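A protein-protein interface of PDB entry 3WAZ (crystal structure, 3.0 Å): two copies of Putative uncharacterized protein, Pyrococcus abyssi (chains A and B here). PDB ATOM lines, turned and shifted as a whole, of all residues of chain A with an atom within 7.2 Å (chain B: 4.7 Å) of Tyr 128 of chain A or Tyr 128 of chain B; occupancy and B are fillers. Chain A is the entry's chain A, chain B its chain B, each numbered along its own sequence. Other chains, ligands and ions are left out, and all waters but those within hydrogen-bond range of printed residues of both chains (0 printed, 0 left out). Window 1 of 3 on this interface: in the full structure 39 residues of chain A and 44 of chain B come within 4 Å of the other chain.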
ATOM      1  N   VAL A  34     -25.582   4.522   2.987  1.00  0.00           N
ATOM      2  CA  VAL A  34     -24.829   5.414   3.865  1.00  0.00           C
ATOM      3  C   VAL A  34     -25.741   6.329   4.687  1.00  0.00           C
ATOM      4  O   VAL A  34     -26.671   6.938   4.158  1.00  0.00           O
ATOM      5  CB  VAL A  34     -23.807   6.257   3.062  1.00  0.00           C
ATOM      6  CG1 VAL A  34     -24.466   6.881   1.838  1.00  0.00           C
ATOM      7  CG2 VAL A  34     -23.163   7.318   3.943  1.00  0.00           C
ATOM      8  N   LEU A 104     -14.437  -9.026  12.839  1.00  0.00           N
ATOM      9  CA  LEU A 104     -14.428  -7.919  11.886  1.00  0.00           C
ATOM     10  C   LEU A 104     -13.173  -7.076  12.062  1.00  0.00           C
ATOM     11  O   LEU A 104     -12.623  -6.550  11.094  1.00  0.00           O
ATOM     12  CB  LEU A 104     -15.658  -7.030  12.066  1.00  0.00           C
ATOM     13  CG  LEU A 104     -15.727  -5.859  11.081  1.00  0.00           C
ATOM     14  CD1 LEU A 104     -16.436  -6.266   9.796  1.00  0.00           C
ATOM     15  CD2 LEU A 104     -16.374  -4.637  11.706  1.00  0.00           C
ATOM     16  N   GLY A 108      -8.892  -5.653   7.365  1.00  0.00           N
ATOM     17  CA  GLY A 108      -8.050  -4.480   7.242  1.00  0.00           C
ATOM     18  C   GLY A 108      -8.624  -3.341   6.423  1.00  0.00           C
ATOM     19  O   GLY A 108      -9.446  -3.545   5.527  1.00  0.00           O
ATOM     20  N   ILE A 109      -8.181  -2.131   6.745  1.00  0.00           N
ATOM     21  CA  ILE A 109      -8.513  -0.947   5.969  1.00  0.00           C
ATOM     22  C   ILE A 109      -7.532  -0.851   4.812  1.00  0.00           C
ATOM     23  O   ILE A 109      -6.349  -1.149   4.970  1.00  0.00           O
ATOM     24  CB  ILE A 109      -8.384   0.327   6.821  1.00  0.00           C
ATOM     25  CG1 ILE A 109      -9.092   0.148   8.166  1.00  0.00           C
ATOM     26  CG2 ILE A 109      -8.933   1.534   6.072  1.00  0.00           C
ATOM     27  CD1 ILE A 109      -8.857   1.287   9.129  1.00  0.00           C
ATOM     28  N   ARG A 110      -8.018  -0.437   3.647  1.00  0.00           N
ATOM     29  CA  ARG A 110      -7.152  -0.305   2.483  1.00  0.00           C
ATOM     30  C   ARG A 110      -7.494   0.923   1.647  1.00  0.00           C
ATOM     31  O   ARG A 110      -8.644   1.360   1.606  1.00  0.00           O
ATOM     32  CB  ARG A 110      -7.209  -1.569   1.623  1.00  0.00           C
ATOM     33  CG  ARG A 110      -8.559  -1.833   0.982  1.00  0.00           C
ATOM     34  CD  ARG A 110      -8.539  -3.132   0.194  1.00  0.00           C
ATOM     35  NE  ARG A 110      -9.728  -3.295  -0.639  1.00  0.00           N
ATOM     36  CZ  ARG A 110     -10.860  -3.856  -0.228  1.00  0.00           C
ATOM     37  NH1 ARG A 110     -10.967  -4.308   1.016  1.00  0.00           N
ATOM     38  NH2 ARG A 110     -11.887  -3.962  -1.059  1.00  0.00           N
ATOM     39  N   ARG A 111      -6.482   1.476   0.991  1.00  0.00           N
ATOM     40  CA  ARG A 111      -6.664   2.625   0.115  1.00  0.00           C
ATOM     41  C   ARG A 111      -6.438   2.217  -1.334  1.00  0.00           C
ATOM     42  O   ARG A 111      -5.308   1.954  -1.745  1.00  0.00           O
ATOM     43  CB  ARG A 111      -5.707   3.752   0.505  1.00  0.00           C
ATOM     44  CG  ARG A 111      -5.684   4.916  -0.469  1.00  0.00           C
ATOM     45  CD  ARG A 111      -4.990   6.122   0.138  1.00  0.00           C
ATOM     46  NE  ARG A 111      -5.726   6.645   1.285  1.00  0.00           N
ATOM     47  CZ  ARG A 111      -5.357   7.710   1.988  1.00  0.00           C
ATOM     48  NH1 ARG A 111      -4.255   8.372   1.662  1.00  0.00           N
ATOM     49  NH2 ARG A 111      -6.090   8.114   3.016  1.00  0.00           N
ATOM     50  N   GLU A 112      -7.518   2.161  -2.104  1.00  0.00           N
ATOM     51  CA  GLU A 112      -7.442   1.714  -3.490  1.00  0.00           C
ATOM     52  C   GLU A 112      -7.338   2.874  -4.473  1.00  0.00           C
ATOM     53  O   GLU A 112      -7.869   3.958  -4.235  1.00  0.00           O
ATOM     54  CB  GLU A 112      -8.640   0.830  -3.837  1.00  0.00           C
ATOM     55  CG  GLU A 112      -8.697  -0.463  -3.041  1.00  0.00           C
ATOM     56  CD  GLU A 112      -9.846  -1.355  -3.466  1.00  0.00           C
ATOM     57  OE1 GLU A 112     -10.628  -0.940  -4.347  1.00  0.00           O
ATOM     58  OE2 GLU A 112      -9.964  -2.471  -2.920  1.00  0.00           O
ATOM     59  N   TYR A 124      -8.233   8.511  -4.948  1.00  0.00           N
ATOM     60  CA  TYR A 124      -8.155   7.212  -4.293  1.00  0.00           C
ATOM     61  C   TYR A 124      -9.436   6.928  -3.522  1.00  0.00           C
ATOM     62  O   TYR A 124     -10.311   7.788  -3.415  1.00  0.00           O
ATOM     63  CB  TYR A 124      -6.960   7.156  -3.342  1.00  0.00           C
ATOM     64  CG  TYR A 124      -5.620   7.153  -4.037  1.00  0.00           C
ATOM     65  CD1 TYR A 124      -5.013   8.340  -4.423  1.00  0.00           C
ATOM     66  CD2 TYR A 124      -4.956   5.962  -4.301  1.00  0.00           C
ATOM     67  CE1 TYR A 124      -3.786   8.342  -5.057  1.00  0.00           C
ATOM     68  CE2 TYR A 124      -3.729   5.954  -4.936  1.00  0.00           C
ATOM     69  CZ  TYR A 124      -3.149   7.146  -5.311  1.00  0.00           C
ATOM     70  OH  TYR A 124      -1.925   7.146  -5.941  1.00  0.00           O
ATOM     71  N   GLU A 125      -9.538   5.719  -2.984  1.00  0.00           N
ATOM     72  CA  GLU A 125     -10.694   5.325  -2.191  1.00  0.00           C
ATOM     73  C   GLU A 125     -10.263   4.634  -0.905  1.00  0.00           C
ATOM     74  O   GLU A 125      -9.606   3.595  -0.942  1.00  0.00           O
ATOM     75  CB  GLU A 125     -11.599   4.388  -2.991  1.00  0.00           C
ATOM     76  CG  GLU A 125     -12.316   5.037  -4.163  1.00  0.00           C
ATOM     77  CD  GLU A 125     -13.183   4.053  -4.926  1.00  0.00           C
ATOM     78  OE1 GLU A 125     -14.037   4.501  -5.720  1.00  0.00           O
ATOM     79  OE2 GLU A 125     -13.009   2.831  -4.731  1.00  0.00           O
ATOM     80  N   ASP A 126     -10.626   5.218   0.233  1.00  0.00           N
ATOM     81  CA  ASP A 126     -10.413   4.570   1.521  1.00  0.00           C
ATOM     82  C   ASP A 126     -11.548   3.591   1.784  1.00  0.00           C
ATOM     83  O   ASP A 126     -12.720   3.964   1.758  1.00  0.00           O
ATOM     84  CB  ASP A 126     -10.310   5.602   2.645  1.00  0.00           C
ATOM     85  CG  ASP A 126      -8.899   6.137   2.817  1.00  0.00           C
ATOM     86  OD1 ASP A 126      -8.069   5.925   1.909  1.00  0.00           O
ATOM     87  OD2 ASP A 126      -8.622   6.772   3.859  1.00  0.00           O
ATOM     88  N   VAL A 127     -11.195   2.334   2.030  1.00  0.00           N
ATOM     89  CA  VAL A 127     -12.188   1.274   2.163  1.00  0.00           C
ATOM     90  C   VAL A 127     -12.213   0.687   3.570  1.00  0.00           C
ATOM     91  O   VAL A 127     -11.240   0.087   4.023  1.00  0.00           O
ATOM     92  CB  VAL A 127     -11.930   0.149   1.150  1.00  0.00           C
ATOM     93  CG1 VAL A 127     -13.052  -0.874   1.196  1.00  0.00           C
ATOM     94  CG2 VAL A 127     -11.789   0.726  -0.247  1.00  0.00           C
ATOM     95  N   TYR A 128     -13.340   0.865   4.254  1.00  0.00           N
ATOM     96  CA  TYR A 128     -13.513   0.354   5.609  1.00  0.00           C
ATOM     97  C   TYR A 128     -14.506  -0.807   5.630  1.00  0.00           C
ATOM     98  O   TYR A 128     -15.606  -0.701   5.087  1.00  0.00           O
ATOM     99  CB  TYR A 128     -13.983   1.471   6.544  1.00  0.00           C
ATOM    100  CG  TYR A 128     -12.985   2.595   6.707  1.00  0.00           C
ATOM    101  CD1 TYR A 128     -12.130   2.637   7.800  1.00  0.00           C
ATOM    102  CD2 TYR A 128     -12.898   3.616   5.771  1.00  0.00           C
ATOM    103  CE1 TYR A 128     -11.215   3.664   7.952  1.00  0.00           C
ATOM    104  CE2 TYR A 128     -11.987   4.646   5.915  1.00  0.00           C
ATOM    105  CZ  TYR A 128     -11.149   4.665   7.008  1.00  0.00           C
ATOM    106  OH  TYR A 128     -10.238   5.685   7.157  1.00  0.00           O
ATOM    107  N   PRO A 129     -14.115  -1.925   6.259  1.00  0.00           N
ATOM    108  CA  PRO A 129     -14.935  -3.141   6.309  1.00  0.00           C
ATOM    109  C   PRO A 129     -16.162  -2.990   7.204  1.00  0.00           C
ATOM    110  O   PRO A 129     -16.103  -2.306   8.225  1.00  0.00           O
ATOM    111  CB  PRO A 129     -13.978  -4.181   6.895  1.00  0.00           C
ATOM    112  CG  PRO A 129     -13.009  -3.393   7.689  1.00  0.00           C
ATOM    113  CD  PRO A 129     -12.826  -2.100   6.951  1.00  0.00           C
ATOM    114  N   VAL A 130     -17.260  -3.629   6.812  1.00  0.00           N
ATOM    115  CA  VAL A 130     -18.517  -3.550   7.548  1.00  0.00           C
ATOM    116  C   VAL A 130     -19.205  -4.913   7.613  1.00  0.00           C
ATOM    117  O   VAL A 130     -19.339  -5.597   6.599  1.00  0.00           O
ATOM    118  CB  VAL A 130     -19.491  -2.538   6.895  1.00  0.00           C
ATOM    119  CG1 VAL A 130     -20.868  -2.616   7.543  1.00  0.00           C
ATOM    120  CG2 VAL A 130     -18.939  -1.123   6.977  1.00  0.00           C
ATOM    121  N   ALA A 131     -19.631  -5.306   8.810  1.00  0.00           N
ATOM    122  CA  ALA A 131     -20.459  -6.494   8.980  1.00  0.00           C
ATOM    123  C   ALA A 131     -21.884  -6.068   9.319  1.00  0.00           C
ATOM    124  O   ALA A 131     -22.096  -5.238  10.202  1.00  0.00           O
ATOM    125  CB  ALA A 131     -19.897  -7.389  10.070  1.00  0.00           C
ATOM    126  N   VAL A 144     -19.082  -1.680  12.236  1.00  0.00           N
ATOM    127  CA  VAL A 144     -18.238  -0.860  11.374  1.00  0.00           C
ATOM    128  C   VAL A 144     -16.859  -0.614  11.976  1.00  0.00           C
ATOM    129  O   VAL A 144     -16.741  -0.204  13.131  1.00  0.00           O
ATOM    130  CB  VAL A 144     -18.902   0.502  11.082  1.00  0.00           C
ATOM    131  CG1 VAL A 144     -17.984   1.383  10.252  1.00  0.00           C
ATOM    132  CG2 VAL A 144     -20.233   0.302  10.378  1.00  0.00           C
ATOM    133  N   LEU A 145     -15.820  -0.868  11.186  1.00  0.00           N
ATOM    134  CA  LEU A 145     -14.458  -0.570  11.603  1.00  0.00           C
ATOM    135  C   LEU A 145     -14.124   0.884  11.293  1.00  0.00           C
ATOM    136  O   LEU A 145     -14.077   1.286  10.130  1.00  0.00           O
ATOM    137  CB  LEU A 145     -13.461  -1.493  10.899  1.00  0.00           C
ATOM    138  CG  LEU A 145     -11.998  -1.313  11.315  1.00  0.00           C
ATOM    139  CD1 LEU A 145     -11.811  -1.708  12.768  1.00  0.00           C
ATOM    140  CD2 LEU A 145     -11.063  -2.106  10.417  1.00  0.00           C
ATOM    141  N   LYS A 146     -13.902   1.669  12.341  1.00  0.00           N
ATOM    142  CA  LYS A 146     -13.514   3.065  12.178  1.00  0.00           C
ATOM    143  C   LYS A 146     -12.672   3.526  13.360  1.00  0.00           C
ATOM    144  O   LYS A 146     -12.531   2.810  14.352  1.00  0.00           O
ATOM    145  CB  LYS A 146     -14.744   3.960  12.026  1.00  0.00           C
ATOM    146  CG  LYS A 146     -15.566   4.104  13.292  1.00  0.00           C
ATOM    147  CD  LYS A 146     -16.653   5.162  13.141  1.00  0.00           C
ATOM    148  CE  LYS A 146     -17.663   4.782  12.072  1.00  0.00           C
ATOM    149  NZ  LYS A 146     -18.744   5.797  11.951  1.00  0.00           N
ATOM    150  N   HIS A 147     -12.119   4.728  13.249  1.00  0.00           N
ATOM    151  CA  HIS A 147     -11.238   5.262  14.278  1.00  0.00           C
ATOM    152  C   HIS A 147     -11.997   5.564  15.564  1.00  0.00           C
ATOM    153  O   HIS A 147     -13.144   6.013  15.529  1.00  0.00           O
ATOM    154  CB  HIS A 147     -10.545   6.525  13.771  1.00  0.00           C
ATOM    155  CG  HIS A 147      -9.332   6.904  14.560  1.00  0.00           C
ATOM    156  ND1 HIS A 147      -9.405   7.463  15.818  1.00  0.00           N
ATOM    157  CD2 HIS A 147      -8.014   6.807  14.268  1.00  0.00           C
ATOM    158  CE1 HIS A 147      -8.184   7.691  16.267  1.00  0.00           C
ATOM    159  NE2 HIS A 147      -7.321   7.302  15.346  1.00  0.00           N
ATOM    160  N   TYR A 154      -8.127   2.001  15.411  1.00  0.00           N
ATOM    161  CA  TYR A 154      -9.433   1.647  14.872  1.00  0.00           C
ATOM    162  C   TYR A 154     -10.083   0.508  15.648  1.00  0.00           C
ATOM    163  O   TYR A 154      -9.424  -0.462  16.020  1.00  0.00           O
ATOM    164  CB  TYR A 154      -9.306   1.269  13.396  1.00  0.00           C
ATOM    165  CG  TYR A 154      -8.665   2.346  12.552  1.00  0.00           C
ATOM    166  CD1 TYR A 154      -7.294   2.354  12.324  1.00  0.00           C
ATOM    167  CD2 TYR A 154      -9.428   3.354  11.985  1.00  0.00           C
ATOM    168  CE1 TYR A 154      -6.706   3.338  11.554  1.00  0.00           C
ATOM    169  CE2 TYR A 154      -8.850   4.342  11.215  1.00  0.00           C
ATOM    170  CZ  TYR A 154      -7.489   4.330  11.003  1.00  0.00           C
ATOM    171  OH  TYR A 154      -6.909   5.313  10.235  1.00  0.00           O
ATOM    172  N   ILE B 109     -20.016   9.353  -0.641  1.00  0.00           N
ATOM    173  CA  ILE B 109     -19.684   8.182   0.155  1.00  0.00           C
ATOM    174  C   ILE B 109     -20.668   7.068  -0.174  1.00  0.00           C
ATOM    175  O   ILE B 109     -21.872   7.307  -0.264  1.00  0.00           O
ATOM    176  CB  ILE B 109     -19.772   8.486   1.664  1.00  0.00           C
ATOM    177  CG1 ILE B 109     -18.925   9.709   2.018  1.00  0.00           C
ATOM    178  CG2 ILE B 109     -19.341   7.276   2.476  1.00  0.00           C
ATOM    179  CD1 ILE B 109     -19.071  10.156   3.459  1.00  0.00           C
ATOM    180  N   TYR B 124     -19.866  -5.851   4.160  1.00  0.00           N
ATOM    181  CA  TYR B 124     -19.964  -4.695   3.280  1.00  0.00           C
ATOM    182  C   TYR B 124     -18.686  -3.875   3.361  1.00  0.00           C
ATOM    183  O   TYR B 124     -17.830  -4.129   4.208  1.00  0.00           O
ATOM    184  CB  TYR B 124     -21.165  -3.828   3.660  1.00  0.00           C
ATOM    185  CG  TYR B 124     -22.501  -4.430   3.293  1.00  0.00           C
ATOM    186  CD1 TYR B 124     -23.132  -5.337   4.132  1.00  0.00           C
ATOM    187  CD2 TYR B 124     -23.135  -4.087   2.106  1.00  0.00           C
ATOM    188  CE1 TYR B 124     -24.355  -5.887   3.799  1.00  0.00           C
ATOM    189  CE2 TYR B 124     -24.357  -4.631   1.766  1.00  0.00           C
ATOM    190  CZ  TYR B 124     -24.962  -5.530   2.615  1.00  0.00           C
ATOM    191  OH  TYR B 124     -26.181  -6.074   2.277  1.00  0.00           O
ATOM    192  N   GLU B 125     -18.561  -2.894   2.475  1.00  0.00           N
ATOM    193  CA  GLU B 125     -17.403  -2.010   2.474  1.00  0.00           C
ATOM    194  C   GLU B 125     -17.830  -0.555   2.332  1.00  0.00           C
ATOM    195  O   GLU B 125     -18.437  -0.172   1.332  1.00  0.00           O
ATOM    196  CB  GLU B 125     -16.439  -2.381   1.344  1.00  0.00           C
ATOM    197  CG  GLU B 125     -15.762  -3.732   1.513  1.00  0.00           C
ATOM    198  CD  GLU B 125     -14.842  -4.072   0.355  1.00  0.00           C
ATOM    199  OE1 GLU B 125     -14.058  -5.037   0.480  1.00  0.00           O
ATOM    200  OE2 GLU B 125     -14.905  -3.376  -0.682  1.00  0.00           O
ATOM    201  N   ASP B 126     -17.523   0.249   3.344  1.00  0.00           N
ATOM    202  CA  ASP B 126     -17.743   1.687   3.270  1.00  0.00           C
ATOM    203  C   ASP B 126     -16.586   2.340   2.529  1.00  0.00           C
ATOM    204  O   ASP B 126     -15.424   2.161   2.894  1.00  0.00           O
ATOM    205  CB  ASP B 126     -17.899   2.288   4.667  1.00  0.00           C
ATOM    206  CG  ASP B 126     -19.309   2.142   5.208  1.00  0.00           C
ATOM    207  OD1 ASP B 126     -19.621   2.774   6.242  1.00  0.00           O
ATOM    208  OD2 ASP B 126     -20.110   1.406   4.593  1.00  0.00           O
ATOM    209  N   VAL B 127     -16.908   3.090   1.481  1.00  0.00           N
ATOM    210  CA  VAL B 127     -15.889   3.668   0.615  1.00  0.00           C
ATOM    211  C   VAL B 127     -15.909   5.192   0.651  1.00  0.00           C
ATOM    212  O   VAL B 127     -16.872   5.821   0.212  1.00  0.00           O
ATOM    213  CB  VAL B 127     -16.065   3.194  -0.837  1.00  0.00           C
ATOM    214  CG1 VAL B 127     -14.911   3.677  -1.694  1.00  0.00           C
ATOM    215  CG2 VAL B 127     -16.171   1.682  -0.887  1.00  0.00           C
ATOM    216  N   TYR B 128     -14.839   5.778   1.178  1.00  0.00           N
ATOM    217  CA  TYR B 128     -14.705   7.229   1.248  1.00  0.00           C
ATOM    218  C   TYR B 128     -13.712   7.719   0.199  1.00  0.00           C
ATOM    219  O   TYR B 128     -12.655   7.116   0.010  1.00  0.00           O
ATOM    220  CB  TYR B 128     -14.254   7.657   2.648  1.00  0.00           C
ATOM    221  CG  TYR B 128     -15.207   7.258   3.754  1.00  0.00           C
ATOM    222  CD1 TYR B 128     -16.173   8.140   4.218  1.00  0.00           C
ATOM    223  CD2 TYR B 128     -15.139   5.999   4.335  1.00  0.00           C
ATOM    224  CE1 TYR B 128     -17.046   7.780   5.229  1.00  0.00           C
ATOM    225  CE2 TYR B 128     -16.007   5.628   5.346  1.00  0.00           C
ATOM    226  CZ  TYR B 128     -16.958   6.523   5.788  1.00  0.00           C
ATOM    227  OH  TYR B 128     -17.825   6.159   6.794  1.00  0.00           O
ATOM    228  N   PRO B 129     -14.051   8.817  -0.494  1.00  0.00           N
ATOM    229  CA  PRO B 129     -13.206   9.354  -1.565  1.00  0.00           C
ATOM    230  C   PRO B 129     -11.966  10.064  -1.031  1.00  0.00           C
ATOM    231  O   PRO B 129     -12.030  10.727   0.003  1.00  0.00           O
ATOM    232  CB  PRO B 129     -14.129  10.354  -2.265  1.00  0.00           C
ATOM    233  CG  PRO B 129     -15.064  10.795  -1.203  1.00  0.00           C
ATOM    234  CD  PRO B 129     -15.286   9.599  -0.317  1.00  0.00           C
ATOM    235  N   VAL B 130     -10.849   9.916  -1.739  1.00  0.00           N
ATOM    236  CA  VAL B 130      -9.585  10.523  -1.339  1.00  0.00           C
ATOM    237  C   VAL B 130      -8.882  11.165  -2.534  1.00  0.00           C
ATOM    238  O   VAL B 130      -8.798  10.567  -3.608  1.00  0.00           O
ATOM    239  CB  VAL B 130      -8.635   9.478  -0.705  1.00  0.00           C
ATOM    240  CG1 VAL B 130      -7.266  10.089  -0.427  1.00  0.00           C
ATOM    241  CG2 VAL B 130      -9.234   8.911   0.571  1.00  0.00           C
ATOM    242  N   LEU B 145     -12.336  12.777   2.639  1.00  0.00           N
ATOM    243  CA  LEU B 145     -13.698  13.025   3.083  1.00  0.00           C
ATOM    244  C   LEU B 145     -14.031  12.094   4.240  1.00  0.00           C
ATOM    245  O   LEU B 145     -14.125  10.878   4.064  1.00  0.00           O
ATOM    246  CB  LEU B 145     -14.688  12.806   1.937  1.00  0.00           C
ATOM    247  CG  LEU B 145     -16.154  13.095   2.269  1.00  0.00           C
ATOM    248  CD1 LEU B 145     -16.324  14.548   2.676  1.00  0.00           C
ATOM    249  CD2 LEU B 145     -17.060  12.759   1.094  1.00  0.00           C
ATOM    250  N   TYR B 154     -20.029  15.211   7.315  1.00  0.00           N
ATOM    251  CA  TYR B 154     -18.724  14.937   6.726  1.00  0.00           C
ATOM    252  C   TYR B 154     -18.160  16.173   6.038  1.00  0.00           C
ATOM    253  O   TYR B 154     -18.903  16.981   5.479  1.00  0.00           O
ATOM    254  CB  TYR B 154     -18.826  13.789   5.718  1.00  0.00           C
ATOM    255  CG  TYR B 154     -19.455  12.535   6.280  1.00  0.00           C
ATOM    256  CD1 TYR B 154     -20.825  12.324   6.196  1.00  0.00           C
ATOM    257  CD2 TYR B 154     -18.679  11.561   6.891  1.00  0.00           C
ATOM    258  CE1 TYR B 154     -21.402  11.178   6.709  1.00  0.00           C
ATOM    259  CE2 TYR B 154     -19.247  10.413   7.409  1.00  0.00           C
ATOM    260  CZ  TYR B 154     -20.609  10.226   7.315  1.00  0.00           C
ATOM    261  OH  TYR B 154     -21.175   9.083   7.829  1.00  0.00           O
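Among the printed residues, merely in contact across the chains: Val 34 of chain A with Ile 109 of chain B (3.4 Å), Arg 111 of chain A with Val 130 of chain B (3.9 Å), Tyr 124 of chain A with Pro 129 of chain B (3.7 Å), Glu 125 of chain A with Val 127 of chain B (3.6 Å), Glu 125 of chain A with Tyr 128 of chain B (3.4 Å), Asp 126 of chain A with Val 127 of chain B (3.4 Å), Asp 126 of chain A with Val 130 of chain B (3.5 Å), Val 127 of chain A with Glu 125 of chain B (3.6 Å), Val 127 of chain A with Asp 126 of chain B (3.4 Å), Tyr 128 of chain A with Glu 125 of chain B (3.4 Å), Tyr 128 of chain A with Tyr 128 of chain B (3.6 Å), Pro 129 of chain A with Tyr 124 of chain B (3.6 Å) and Val 130 of chain A with Asp 126 of chain B (3.7 Å).
Printed residues of chain B within 4 Å of Tyr 128 of chain A: Glu 125, Asp 126 and Tyr 128. Printed residues of chain B within 4 Å of Arg 111 of chain A: Val 130. Of the printed residues of chain A, Tyr 124 of chain B touches Pro 129 (3.6 Å) and Val 130 (2.5 Å). Printed residues of chain B within 4 Å of Glu 125 of chain A: Val 127 and Tyr 128. Printed residues of chain A within 4 Å of Val 130 of chain B: Arg 111, Tyr 124 and Asp 126. The nearest residue of chain A that does not touch Tyr 128 of chain B is Tyr 124 of chain A (4.2 Å). The nearest printed residue of chain B that does not touch Val 130 of chain A is Glu 125 of chain B (4.5 Å).
O of Arg 110 of chain A is in hydrogen-bond range of N of Val 127 of chain A (2.8 Å). The backbone NH (N) of Leu 145 of chain A is in hydrogen-bond range of the backbone carbonyl oxygen (O) of Pro 129 of chain A, at 3.3 Å. The backbone carbonyl oxygen of Pro 129 of chain B is in hydrogen-bond range of the backbone NH of Leu 145 of chain B, 3.4 Å away. The guanidinium group (NE) of Arg 111 of chain A lies within salt-bridge range of the side-chain carboxylate (OD1) of Asp 126 of chain A. The guanidinium group of Arg 110 of chain A is in salt-bridge range of the side-chain carboxylate of Glu 112 of chain A (2.4 Å). O of Glu 112 of chain A sits at hydrogen-bond distance from N of Glu 125 of chain A (2.7 Å).
Hydrophobic or aromatic side chains of chain B that line the printed part of chain A: Tyr 124, Val 127, Tyr 128 and Val 130. Along chain B the printed residues that touch a printed residue of chain A span positions 109 to 130. Of the 20 printed residues of chain A, 10 touch a printed residue of chain B. Printed residues of chain A that touch a printed residue of chain B: Val 34, Arg 110, Arg 111, Tyr 124, Glu 125, Asp 126, Val 127, Tyr 128, Pro 129 and Val 130.
The backbone carbonyl oxygen (O) of Asp 126 of chain A sits close to the backbone carbonyl oxygen (O) of Asp 126 of chain B, 3.4 Å away. The side-chain carboxylate of Glu 125 of chain B lies within salt-bridge range of the guanidinium group of Arg 110 of chain A (2.9 Å). N of Tyr 124 of chain B lies within hydrogen-bond range of O of Val 130 of chain A, 2.5 Å away. The backbone NH of Tyr 124 of chain A sits at hydrogen-bond distance from the backbone carbonyl oxygen of Val 130 of chain B. The backbone NH (N) of Asp 126 of chain A lies within hydrogen-bond range of the backbone carbonyl oxygen (O) of Tyr 128 of chain B (2.8 Å). The backbone carbonyl oxygen of Tyr 128 of chain A sits at hydrogen-bond distance from the backbone NH of Asp 126 of chain B.
Tyr 124 of chain A touches Pro 129 of chain B, and with the chains exchanged Pro 129 of chain A touches Tyr 124 of chain B. Glu 125 of chain A touches Val 127 of chain B, and with the chains exchanged Val 127 of chain A touches Glu 125 of chain B. Asp 126 of chain A touches its own counterpart, Asp 126 of chain B. Asp 126 of chain A touches Tyr 128 of chain B, and with the chains exchanged Tyr 128 of chain A touches Asp 126 of chain B.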
